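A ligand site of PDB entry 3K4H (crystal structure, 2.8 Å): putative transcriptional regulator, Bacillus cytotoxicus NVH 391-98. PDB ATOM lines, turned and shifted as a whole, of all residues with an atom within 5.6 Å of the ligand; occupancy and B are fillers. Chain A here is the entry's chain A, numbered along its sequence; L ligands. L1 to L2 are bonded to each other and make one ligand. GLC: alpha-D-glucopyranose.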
ATOM      1  N   PRO A  16      14.322   9.089 -17.866  1.00  0.00           N
ATOM      2  CA  PRO A  16      13.559   9.148 -19.106  1.00  0.00           C
ATOM      3  C   PRO A  16      13.651  10.508 -19.770  1.00  0.00           C
ATOM      4  O   PRO A  16      13.253  10.641 -20.924  1.00  0.00           O
ATOM      5  CB  PRO A  16      12.130   8.893 -18.671  1.00  0.00           C
ATOM      6  CG  PRO A  16      12.174   8.560 -17.264  1.00  0.00           C
ATOM      7  CD  PRO A  16      13.434   8.990 -16.687  1.00  0.00           C
ATOM      8  N   LYS A  21      13.523  17.759 -15.210  1.00  0.00           N
ATOM      9  CA  LYS A  21      12.138  17.280 -15.217  1.00  0.00           C
ATOM     10  C   LYS A  21      11.989  16.143 -14.180  1.00  0.00           C
ATOM     11  O   LYS A  21      11.029  16.123 -13.409  1.00  0.00           O
ATOM     12  CB  LYS A  21      11.684  16.847 -16.616  1.00  0.00           C
ATOM     13  CG  LYS A  21      10.149  16.666 -16.825  1.00  0.00           C
ATOM     14  CD  LYS A  21       9.450  15.529 -15.970  1.00  0.00           C
ATOM     15  CE  LYS A  21       9.832  14.083 -16.426  1.00  0.00           C
ATOM     16  NZ  LYS A  21       9.372  12.966 -15.513  1.00  0.00           N
ATOM     17  N   ASN A  25       9.512  15.263 -10.078  1.00  0.00           N
ATOM     18  CA  ASN A  25       8.663  14.137  -9.763  1.00  0.00           C
ATOM     19  C   ASN A  25       9.191  13.426  -8.529  1.00  0.00           C
ATOM     20  O   ASN A  25      10.325  12.963  -8.532  1.00  0.00           O
ATOM     21  CB  ASN A  25       8.549  13.174 -10.938  1.00  0.00           C
ATOM     22  CG  ASN A  25       7.565  12.080 -10.662  1.00  0.00           C
ATOM     23  OD1 ASN A  25       7.429  11.648  -9.521  1.00  0.00           O
ATOM     24  ND2 ASN A  25       6.842  11.634 -11.667  1.00  0.00           N
ATOM     25  N   PHE A  27       9.005  10.635  -7.424  1.00  0.00           N
ATOM     26  CA  PHE A  27       9.486   9.267  -7.621  1.00  0.00           C
ATOM     27  C   PHE A  27      11.031   9.157  -7.611  1.00  0.00           C
ATOM     28  O   PHE A  27      11.612   8.219  -6.999  1.00  0.00           O
ATOM     29  CB  PHE A  27       8.939   8.627  -8.895  1.00  0.00           C
ATOM     30  CG  PHE A  27       9.440   7.225  -9.115  1.00  0.00           C
ATOM     31  CD1 PHE A  27       8.786   6.145  -8.551  1.00  0.00           C
ATOM     32  CD2 PHE A  27      10.600   6.999  -9.843  1.00  0.00           C
ATOM     33  CE1 PHE A  27       9.263   4.832  -8.716  1.00  0.00           C
ATOM     34  CE2 PHE A  27      11.091   5.684 -10.006  1.00  0.00           C
ATOM     35  CZ  PHE A  27      10.416   4.609  -9.439  1.00  0.00           C
ATOM     36  N   PHE A  28      11.676  10.097  -8.296  1.00  0.00           N
ATOM     37  CA  PHE A  28      13.102   9.978  -8.543  1.00  0.00           C
ATOM     38  C   PHE A  28      14.070  10.201  -7.379  1.00  0.00           C
ATOM     39  O   PHE A  28      14.976   9.380  -7.203  1.00  0.00           O
ATOM     40  CB  PHE A  28      13.482  10.719  -9.812  1.00  0.00           C
ATOM     41  CG  PHE A  28      12.797  10.152 -11.011  1.00  0.00           C
ATOM     42  CD1 PHE A  28      11.648  10.754 -11.518  1.00  0.00           C
ATOM     43  CD2 PHE A  28      13.244   8.963 -11.590  1.00  0.00           C
ATOM     44  CE1 PHE A  28      10.973  10.190 -12.619  1.00  0.00           C
ATOM     45  CE2 PHE A  28      12.589   8.398 -12.681  1.00  0.00           C
ATOM     46  CZ  PHE A  28      11.442   9.010 -13.192  1.00  0.00           C
ATOM     47  N   LEU A  76      16.338   4.083 -14.928  1.00  0.00           N
ATOM     48  CA  LEU A  76      15.265   4.379 -13.968  1.00  0.00           C
ATOM     49  C   LEU A  76      13.883   4.343 -14.593  1.00  0.00           C
ATOM     50  O   LEU A  76      12.900   4.801 -13.999  1.00  0.00           O
ATOM     51  CB  LEU A  76      15.480   5.723 -13.295  1.00  0.00           C
ATOM     52  CG  LEU A  76      16.506   5.749 -12.165  1.00  0.00           C
ATOM     53  CD1 LEU A  76      16.547   4.388 -11.588  1.00  0.00           C
ATOM     54  CD2 LEU A  76      17.886   6.114 -12.676  1.00  0.00           C
ATOM     55  N   TYR A  77      13.825   3.796 -15.785  1.00  0.00           N
ATOM     56  CA  TYR A  77      12.603   3.801 -16.541  1.00  0.00           C
ATOM     57  C   TYR A  77      12.626   2.633 -17.535  1.00  0.00           C
ATOM     58  O   TYR A  77      13.685   2.004 -17.732  1.00  0.00           O
ATOM     59  CB  TYR A  77      12.462   5.122 -17.278  1.00  0.00           C
ATOM     60  CG  TYR A  77      13.399   5.232 -18.435  1.00  0.00           C
ATOM     61  CD1 TYR A  77      14.733   5.560 -18.245  1.00  0.00           C
ATOM     62  CD2 TYR A  77      12.948   4.978 -19.727  1.00  0.00           C
ATOM     63  CE1 TYR A  77      15.593   5.660 -19.320  1.00  0.00           C
ATOM     64  CE2 TYR A  77      13.801   5.076 -20.809  1.00  0.00           C
ATOM     65  CZ  TYR A  77      15.126   5.413 -20.601  1.00  0.00           C
ATOM     66  OH  TYR A  77      15.990   5.495 -21.662  1.00  0.00           O
ATOM     67  N   SER A  78      11.470   2.353 -18.154  1.00  0.00           N
ATOM     68  CA  SER A  78      11.357   1.330 -19.170  1.00  0.00           C
ATOM     69  C   SER A  78      10.443   1.726 -20.300  1.00  0.00           C
ATOM     70  O   SER A  78       9.207   1.688 -20.183  1.00  0.00           O
ATOM     71  CB  SER A  78      10.907   0.016 -18.583  1.00  0.00           C
ATOM     72  OG  SER A  78      10.641  -0.882 -19.629  1.00  0.00           O
ATOM     73  N   ILE A  98      14.647  -0.618 -13.992  1.00  0.00           N
ATOM     74  CA  ILE A  98      13.560  -0.451 -13.007  1.00  0.00           C
ATOM     75  C   ILE A  98      12.268  -0.365 -13.815  1.00  0.00           C
ATOM     76  O   ILE A  98      11.935   0.693 -14.331  1.00  0.00           O
ATOM     77  CB  ILE A  98      13.744   0.809 -12.077  1.00  0.00           C
ATOM     78  CG1 ILE A  98      15.120   0.821 -11.375  1.00  0.00           C
ATOM     79  CG2 ILE A  98      12.575   0.926 -11.064  1.00  0.00           C
ATOM     80  CD1 ILE A  98      15.139   1.539 -10.000  1.00  0.00           C
ATOM     81  N   GLY A  99      11.584  -1.480 -13.977  1.00  0.00           N
ATOM     82  CA  GLY A  99      10.445  -1.604 -14.897  1.00  0.00           C
ATOM     83  C   GLY A  99      10.570  -2.830 -15.792  1.00  0.00           C
ATOM     84  O   GLY A  99      11.681  -3.302 -16.066  1.00  0.00           O
ATOM     85  N   LYS A 100       9.443  -3.374 -16.232  1.00  0.00           N
ATOM     86  CA  LYS A 100       9.409  -4.482 -17.178  1.00  0.00           C
ATOM     87  C   LYS A 100       9.990  -4.059 -18.537  1.00  0.00           C
ATOM     88  O   LYS A 100       9.707  -2.966 -19.023  1.00  0.00           O
ATOM     89  CB  LYS A 100       7.973  -4.895 -17.382  1.00  0.00           C
ATOM     90  CG  LYS A 100       7.762  -6.350 -17.594  1.00  0.00           C
ATOM     91  CD  LYS A 100       6.273  -6.677 -17.532  1.00  0.00           C
ATOM     92  CE  LYS A 100       5.559  -6.170 -18.764  1.00  0.00           C
ATOM     93  NZ  LYS A 100       4.137  -6.565 -18.678  1.00  0.00           N
ATOM     94  N   VAL A 111      13.951  -4.826 -12.054  1.00  0.00           N
ATOM     95  CA  VAL A 111      13.247  -4.704 -10.800  1.00  0.00           C
ATOM     96  C   VAL A 111      11.923  -4.017 -11.043  1.00  0.00           C
ATOM     97  O   VAL A 111      11.873  -3.117 -11.794  1.00  0.00           O
ATOM     98  CB  VAL A 111      14.018  -3.887  -9.849  1.00  0.00           C
ATOM     99  CG1 VAL A 111      13.373  -3.913  -8.586  1.00  0.00           C
ATOM    100  CG2 VAL A 111      15.315  -4.444  -9.704  1.00  0.00           C
ATOM    101  N   ASP A 112      10.838  -4.510 -10.504  1.00  0.00           N
ATOM    102  CA  ASP A 112       9.558  -3.941 -10.812  1.00  0.00           C
ATOM    103  C   ASP A 112       8.560  -4.241  -9.762  1.00  0.00           C
ATOM    104  O   ASP A 112       8.847  -4.972  -8.905  1.00  0.00           O
ATOM    105  CB  ASP A 112       9.079  -4.479 -12.127  1.00  0.00           C
ATOM    106  CG  ASP A 112       8.020  -3.669 -12.729  1.00  0.00           C
ATOM    107  OD1 ASP A 112       7.834  -2.539 -12.333  1.00  0.00           O
ATOM    108  OD2 ASP A 112       7.353  -4.166 -13.612  1.00  0.00           O
ATOM    109  N   ASN A 113       7.421  -3.612  -9.778  1.00  0.00           N
ATOM    110  CA  ASN A 113       6.303  -4.054  -8.996  1.00  0.00           C
ATOM    111  C   ASN A 113       5.387  -4.822  -9.887  1.00  0.00           C
ATOM    112  O   ASN A 113       5.442  -4.684 -11.043  1.00  0.00           O
ATOM    113  CB  ASN A 113       5.499  -2.908  -8.475  1.00  0.00           C
ATOM    114  CG  ASN A 113       6.291  -1.844  -7.928  1.00  0.00           C
ATOM    115  OD1 ASN A 113       6.565  -0.900  -8.578  1.00  0.00           O
ATOM    116  ND2 ASN A 113       6.581  -1.948  -6.688  1.00  0.00           N
ATOM    117  N   ASN A 115       2.758  -4.419 -11.420  1.00  0.00           N
ATOM    118  CA  ASN A 115       1.867  -3.364 -11.805  1.00  0.00           C
ATOM    119  C   ASN A 115       0.561  -3.850 -12.411  1.00  0.00           C
ATOM    120  O   ASN A 115      -0.482  -3.250 -12.195  1.00  0.00           O
ATOM    121  CB  ASN A 115       2.588  -2.471 -12.786  1.00  0.00           C
ATOM    122  CG  ASN A 115       3.501  -1.509 -12.106  1.00  0.00           C
ATOM    123  OD1 ASN A 115       3.098  -0.892 -11.122  1.00  0.00           O
ATOM    124  ND2 ASN A 115       4.733  -1.381 -12.600  1.00  0.00           N
ATOM    125  N   LEU A 143       5.640   3.977 -22.332  1.00  0.00           N
ATOM    126  CA  LEU A 143       6.207   3.470 -21.082  1.00  0.00           C
ATOM    127  C   LEU A 143       5.511   2.205 -20.602  1.00  0.00           C
ATOM    128  O   LEU A 143       4.292   2.071 -20.705  1.00  0.00           O
ATOM    129  CB  LEU A 143       6.185   4.521 -19.997  1.00  0.00           C
ATOM    130  CG  LEU A 143       7.082   5.735 -20.197  1.00  0.00           C
ATOM    131  CD1 LEU A 143       7.268   6.378 -18.856  1.00  0.00           C
ATOM    132  CD2 LEU A 143       8.439   5.337 -20.738  1.00  0.00           C
ATOM    133  N   VAL A 145       5.250   0.773 -17.541  1.00  0.00           N
ATOM    134  CA  VAL A 145       4.440   0.903 -16.344  1.00  0.00           C
ATOM    135  C   VAL A 145       3.010   1.387 -16.693  1.00  0.00           C
ATOM    136  O   VAL A 145       2.043   0.914 -16.099  1.00  0.00           O
ATOM    137  CB  VAL A 145       5.120   1.785 -15.289  1.00  0.00           C
ATOM    138  CG1 VAL A 145       5.346   3.220 -15.803  1.00  0.00           C
ATOM    139  CG2 VAL A 145       4.283   1.787 -14.015  1.00  0.00           C
ATOM    140  N   ARG A 149      -0.356  -0.946 -16.155  1.00  0.00           N
ATOM    141  CA  ARG A 149      -1.401  -0.372 -15.307  1.00  0.00           C
ATOM    142  C   ARG A 149      -2.706  -0.237 -16.074  1.00  0.00           C
ATOM    143  O   ARG A 149      -3.763  -0.678 -15.583  1.00  0.00           O
ATOM    144  CB  ARG A 149      -0.943   0.929 -14.658  1.00  0.00           C
ATOM    145  CG  ARG A 149      -0.091   0.635 -13.458  1.00  0.00           C
ATOM    146  CD  ARG A 149       0.459   1.841 -12.788  1.00  0.00           C
ATOM    147  NE  ARG A 149       1.538   1.428 -11.888  1.00  0.00           N
ATOM    148  CZ  ARG A 149       2.461   2.237 -11.384  1.00  0.00           C
ATOM    149  NH1 ARG A 149       2.469   3.519 -11.653  1.00  0.00           N
ATOM    150  NH2 ARG A 149       3.407   1.743 -10.593  1.00  0.00           N
ATOM    151  N   PHE A 174       3.393  13.164 -16.766  1.00  0.00           N
ATOM    152  CA  PHE A 174       3.066  13.188 -15.360  1.00  0.00           C
ATOM    153  C   PHE A 174       3.366  14.519 -14.796  1.00  0.00           C
ATOM    154  O   PHE A 174       4.468  14.812 -14.521  1.00  0.00           O
ATOM    155  CB  PHE A 174       4.061  12.335 -14.640  1.00  0.00           C
ATOM    156  CG  PHE A 174       4.184  10.977 -15.159  1.00  0.00           C
ATOM    157  CD1 PHE A 174       3.290  10.026 -14.831  1.00  0.00           C
ATOM    158  CD2 PHE A 174       5.235  10.631 -15.942  1.00  0.00           C
ATOM    159  CE1 PHE A 174       3.420   8.787 -15.289  1.00  0.00           C
ATOM    160  CE2 PHE A 174       5.355   9.387 -16.390  1.00  0.00           C
ATOM    161  CZ  PHE A 174       4.454   8.474 -16.078  1.00  0.00           C
ATOM    162  N   THR A 199      -2.148   6.997 -12.696  1.00  0.00           N
ATOM    163  CA  THR A 199      -0.958   6.152 -12.624  1.00  0.00           C
ATOM    164  C   THR A 199       0.206   6.841 -11.887  1.00  0.00           C
ATOM    165  O   THR A 199       1.236   6.223 -11.687  1.00  0.00           O
ATOM    166  CB  THR A 199      -0.500   5.725 -14.002  1.00  0.00           C
ATOM    167  OG1 THR A 199      -0.328   6.888 -14.812  1.00  0.00           O
ATOM    168  CG2 THR A 199      -1.525   4.817 -14.651  1.00  0.00           C
ATOM    169  N   ASP A 200      -0.004   8.095 -11.458  1.00  0.00           N
ATOM    170  CA  ASP A 200       1.001   8.871 -10.738  1.00  0.00           C
ATOM    171  C   ASP A 200       0.360   9.944  -9.834  1.00  0.00           C
ATOM    172  O   ASP A 200      -0.486  10.716 -10.290  1.00  0.00           O
ATOM    173  CB  ASP A 200       1.934   9.530 -11.755  1.00  0.00           C
ATOM    174  CG  ASP A 200       3.074  10.278 -11.104  1.00  0.00           C
ATOM    175  OD1 ASP A 200       4.212   9.820 -11.298  1.00  0.00           O
ATOM    176  OD2 ASP A 200       2.859  11.312 -10.423  1.00  0.00           O
ATOM    177  N   PHE A 227      -1.212   6.331  -7.702  1.00  0.00           N
ATOM    178  CA  PHE A 227      -0.095   5.464  -7.431  1.00  0.00           C
ATOM    179  C   PHE A 227       1.095   6.188  -6.910  1.00  0.00           C
ATOM    180  O   PHE A 227       1.301   7.292  -7.216  1.00  0.00           O
ATOM    181  CB  PHE A 227       0.358   4.828  -8.706  1.00  0.00           C
ATOM    182  CG  PHE A 227      -0.261   3.537  -8.993  1.00  0.00           C
ATOM    183  CD1 PHE A 227       0.354   2.399  -8.674  1.00  0.00           C
ATOM    184  CD2 PHE A 227      -1.414   3.456  -9.657  1.00  0.00           C
ATOM    185  CE1 PHE A 227      -0.213   1.227  -8.964  1.00  0.00           C
ATOM    186  CE2 PHE A 227      -1.963   2.280  -9.921  1.00  0.00           C
ATOM    187  CZ  PHE A 227      -1.368   1.175  -9.579  1.00  0.00           C
ATOM    188  N   ASN A 228       1.919   5.501  -6.147  1.00  0.00           N
ATOM    189  CA  ASN A 228       3.176   5.978  -5.618  1.00  0.00           C
ATOM    190  C   ASN A 228       3.319   6.622  -4.265  1.00  0.00           C
ATOM    191  O   ASN A 228       4.381   6.704  -3.791  1.00  0.00           O
ATOM    192  CB  ASN A 228       3.601   7.101  -6.528  1.00  0.00           C
ATOM    193  CG  ASN A 228       4.210   6.664  -7.806  1.00  0.00           C
ATOM    194  OD1 ASN A 228       4.613   7.470  -8.590  1.00  0.00           O
ATOM    195  ND2 ASN A 228       4.275   5.393  -8.029  1.00  0.00           N
ATOM    196  N   VAL A 245       4.210   1.699  -3.502  1.00  0.00           N
ATOM    197  CA  VAL A 245       4.838   0.935  -4.540  1.00  0.00           C
ATOM    198  C   VAL A 245       6.304   0.768  -4.104  1.00  0.00           C
ATOM    199  O   VAL A 245       7.124   0.209  -4.817  1.00  0.00           O
ATOM    200  CB  VAL A 245       4.631   1.726  -5.839  1.00  0.00           C
ATOM    201  CG1 VAL A 245       5.900   2.456  -6.294  1.00  0.00           C
ATOM    202  CG2 VAL A 245       4.036   0.878  -6.908  1.00  0.00           C
ATOM    203  N   LEU A 250      12.639  -0.440  -4.576  1.00  0.00           N
ATOM    204  CA  LEU A 250      12.874  -0.583  -5.998  1.00  0.00           C
ATOM    205  C   LEU A 250      14.305  -0.156  -6.286  1.00  0.00           C
ATOM    206  O   LEU A 250      15.003  -0.826  -7.005  1.00  0.00           O
ATOM    207  CB  LEU A 250      11.902   0.278  -6.833  1.00  0.00           C
ATOM    208  CG  LEU A 250      10.421  -0.080  -6.970  1.00  0.00           C
ATOM    209  CD1 LEU A 250       9.738   0.994  -7.817  1.00  0.00           C
ATOM    210  CD2 LEU A 250      10.161  -1.474  -7.567  1.00  0.00           C
HETATM  211  C1  GLC L   1       6.465   8.043 -12.186  1.00  0.00           C
HETATM  212  C2  GLC L   1       7.817   7.892 -12.882  1.00  0.00           C
HETATM  213  C3  GLC L   1       7.909   6.523 -13.505  1.00  0.00           C
HETATM  214  C4  GLC L   1       7.786   5.528 -12.361  1.00  0.00           C
HETATM  215  C5  GLC L   1       6.370   5.611 -11.796  1.00  0.00           C
HETATM  216  C6  GLC L   1       6.231   4.681 -10.571  1.00  0.00           C
HETATM  217  O1  GLC L   1       5.479   8.260 -13.163  1.00  0.00           O
HETATM  218  O2  GLC L   1       7.940   8.861 -13.888  1.00  0.00           O
HETATM  219  O3  GLC L   1       9.131   6.400 -14.215  1.00  0.00           O
HETATM  220  O4  GLC L   1       8.057   4.205 -12.774  1.00  0.00           O
HETATM  221  O5  GLC L   1       6.059   6.935 -11.402  1.00  0.00           O
HETATM  222  O6  GLC L   1       4.916   4.202 -10.398  1.00  0.00           O
HETATM  223  C1  GLC L   2       9.216   3.568 -12.268  1.00  0.00           C
HETATM  224  C2  GLC L   2       9.959   3.013 -13.475  1.00  0.00           C
HETATM  225  C3  GLC L   2       9.021   2.003 -14.123  1.00  0.00           C
HETATM  226  C4  GLC L   2       8.645   0.888 -13.136  1.00  0.00           C
HETATM  227  C5  GLC L   2       8.099   1.480 -11.851  1.00  0.00           C
HETATM  228  C6  GLC L   2       7.908   0.369 -10.850  1.00  0.00           C
HETATM  229  O2  GLC L   2      10.228   4.077 -14.360  1.00  0.00           O
HETATM  230  O3  GLC L   2       9.648   1.573 -15.312  1.00  0.00           O
HETATM  231  O4  GLC L   2       7.564   0.139 -13.584  1.00  0.00           O
HETATM  232  O5  GLC L   2       8.944   2.515 -11.356  1.00  0.00           O
HETATM  233  O6  GLC L   2       6.517   0.216 -10.709  1.00  0.00           O
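An oxygen (O6) of GLC L2 sits at hydrogen-bond distance from the side-chain amide oxygen of Asn 113 (2.4 Å).
O3 of GLC L2 is in hydrogen-bond range of O of Ile 98 (2.6 Å).
An oxygen (O6) of GLC L1 is in hydrogen-bond range of the side-chain amide nitrogen of Asn 228, at 2.7 Å.
The side-chain carboxylate of Asp 200 is in hydrogen-bond range of an oxygen (O1) of GLC L1 (2.7 Å).
O2 of GLC L2 lies within hydrogen-bond range of O of Leu 76, 2.8 Å away.
The guanidinium group (NH1) of Arg 149 lies within hydrogen-bond range of an oxygen (O6) of GLC L1, at 2.8 Å.
An oxygen (O4) of GLC L2 is in hydrogen-bond range of the side-chain carboxylate (OD1) of Asp 112, at 3.0 Å.
ND2 of Asn 115 lies within hydrogen-bond range of O6 of GLC L2, 3.1 Å away.
The backbone NH (N) of Ser 78 is in hydrogen-bond range of an oxygen (O3) of GLC L2 (3.5 Å).
ND2 of Asn 113 lies within hydrogen-bond range of O of Val 245 (2.9 Å).
OD1 of Asp 200 sits at hydrogen-bond distance from ND2 of Asn 25 (3.2 Å).
The side-chain amide oxygen (OD1) of Asn 115 lies within hydrogen-bond range of the guanidinium group (NH2) of Arg 149, 2.7 Å away.
O of Thr 199 lies within hydrogen-bond range of NH1 of Arg 149, 3.0 Å away.
ND2 of Asn 115 lies within hydrogen-bond range of OD1 of Asp 112, at 3.3 Å.
OD2 of Asp 112 sits at hydrogen-bond distance from N of Lys 100 (3.4 Å).
N of Phe 27 is in hydrogen-bond range of OD1 of Asn 25 (2.8 Å).
N of Gly 99 lies within hydrogen-bond range of O of Val 111 (2.7 Å).
Merely in contact with the ligand: Phe 174 (3.0 Å), Phe 27 (3.2 Å), Tyr 77 (3.2 Å), Gly 99 (3.3 Å), Val 145 (3.4 Å), Phe 28 (3.5 Å), Leu 250 (3.6 Å) and Asn 25 (3.6 Å).
Hydrophobic or aromatic side chains that line the ligand: Phe 27, Phe 28, Tyr 77, Ile 98, Val 145, Phe 174 and Leu 250.
17 residues have an atom within 4 Å of the ligand: Asn 25, Phe 27, Phe 28, Leu 76, Tyr 77, Ser 78, Ile 98, Gly 99, Asp 112, Asn 113, Asn 115, Val 145, Arg 149, Phe 174, Asp 200, Asn 228 and Leu 250.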
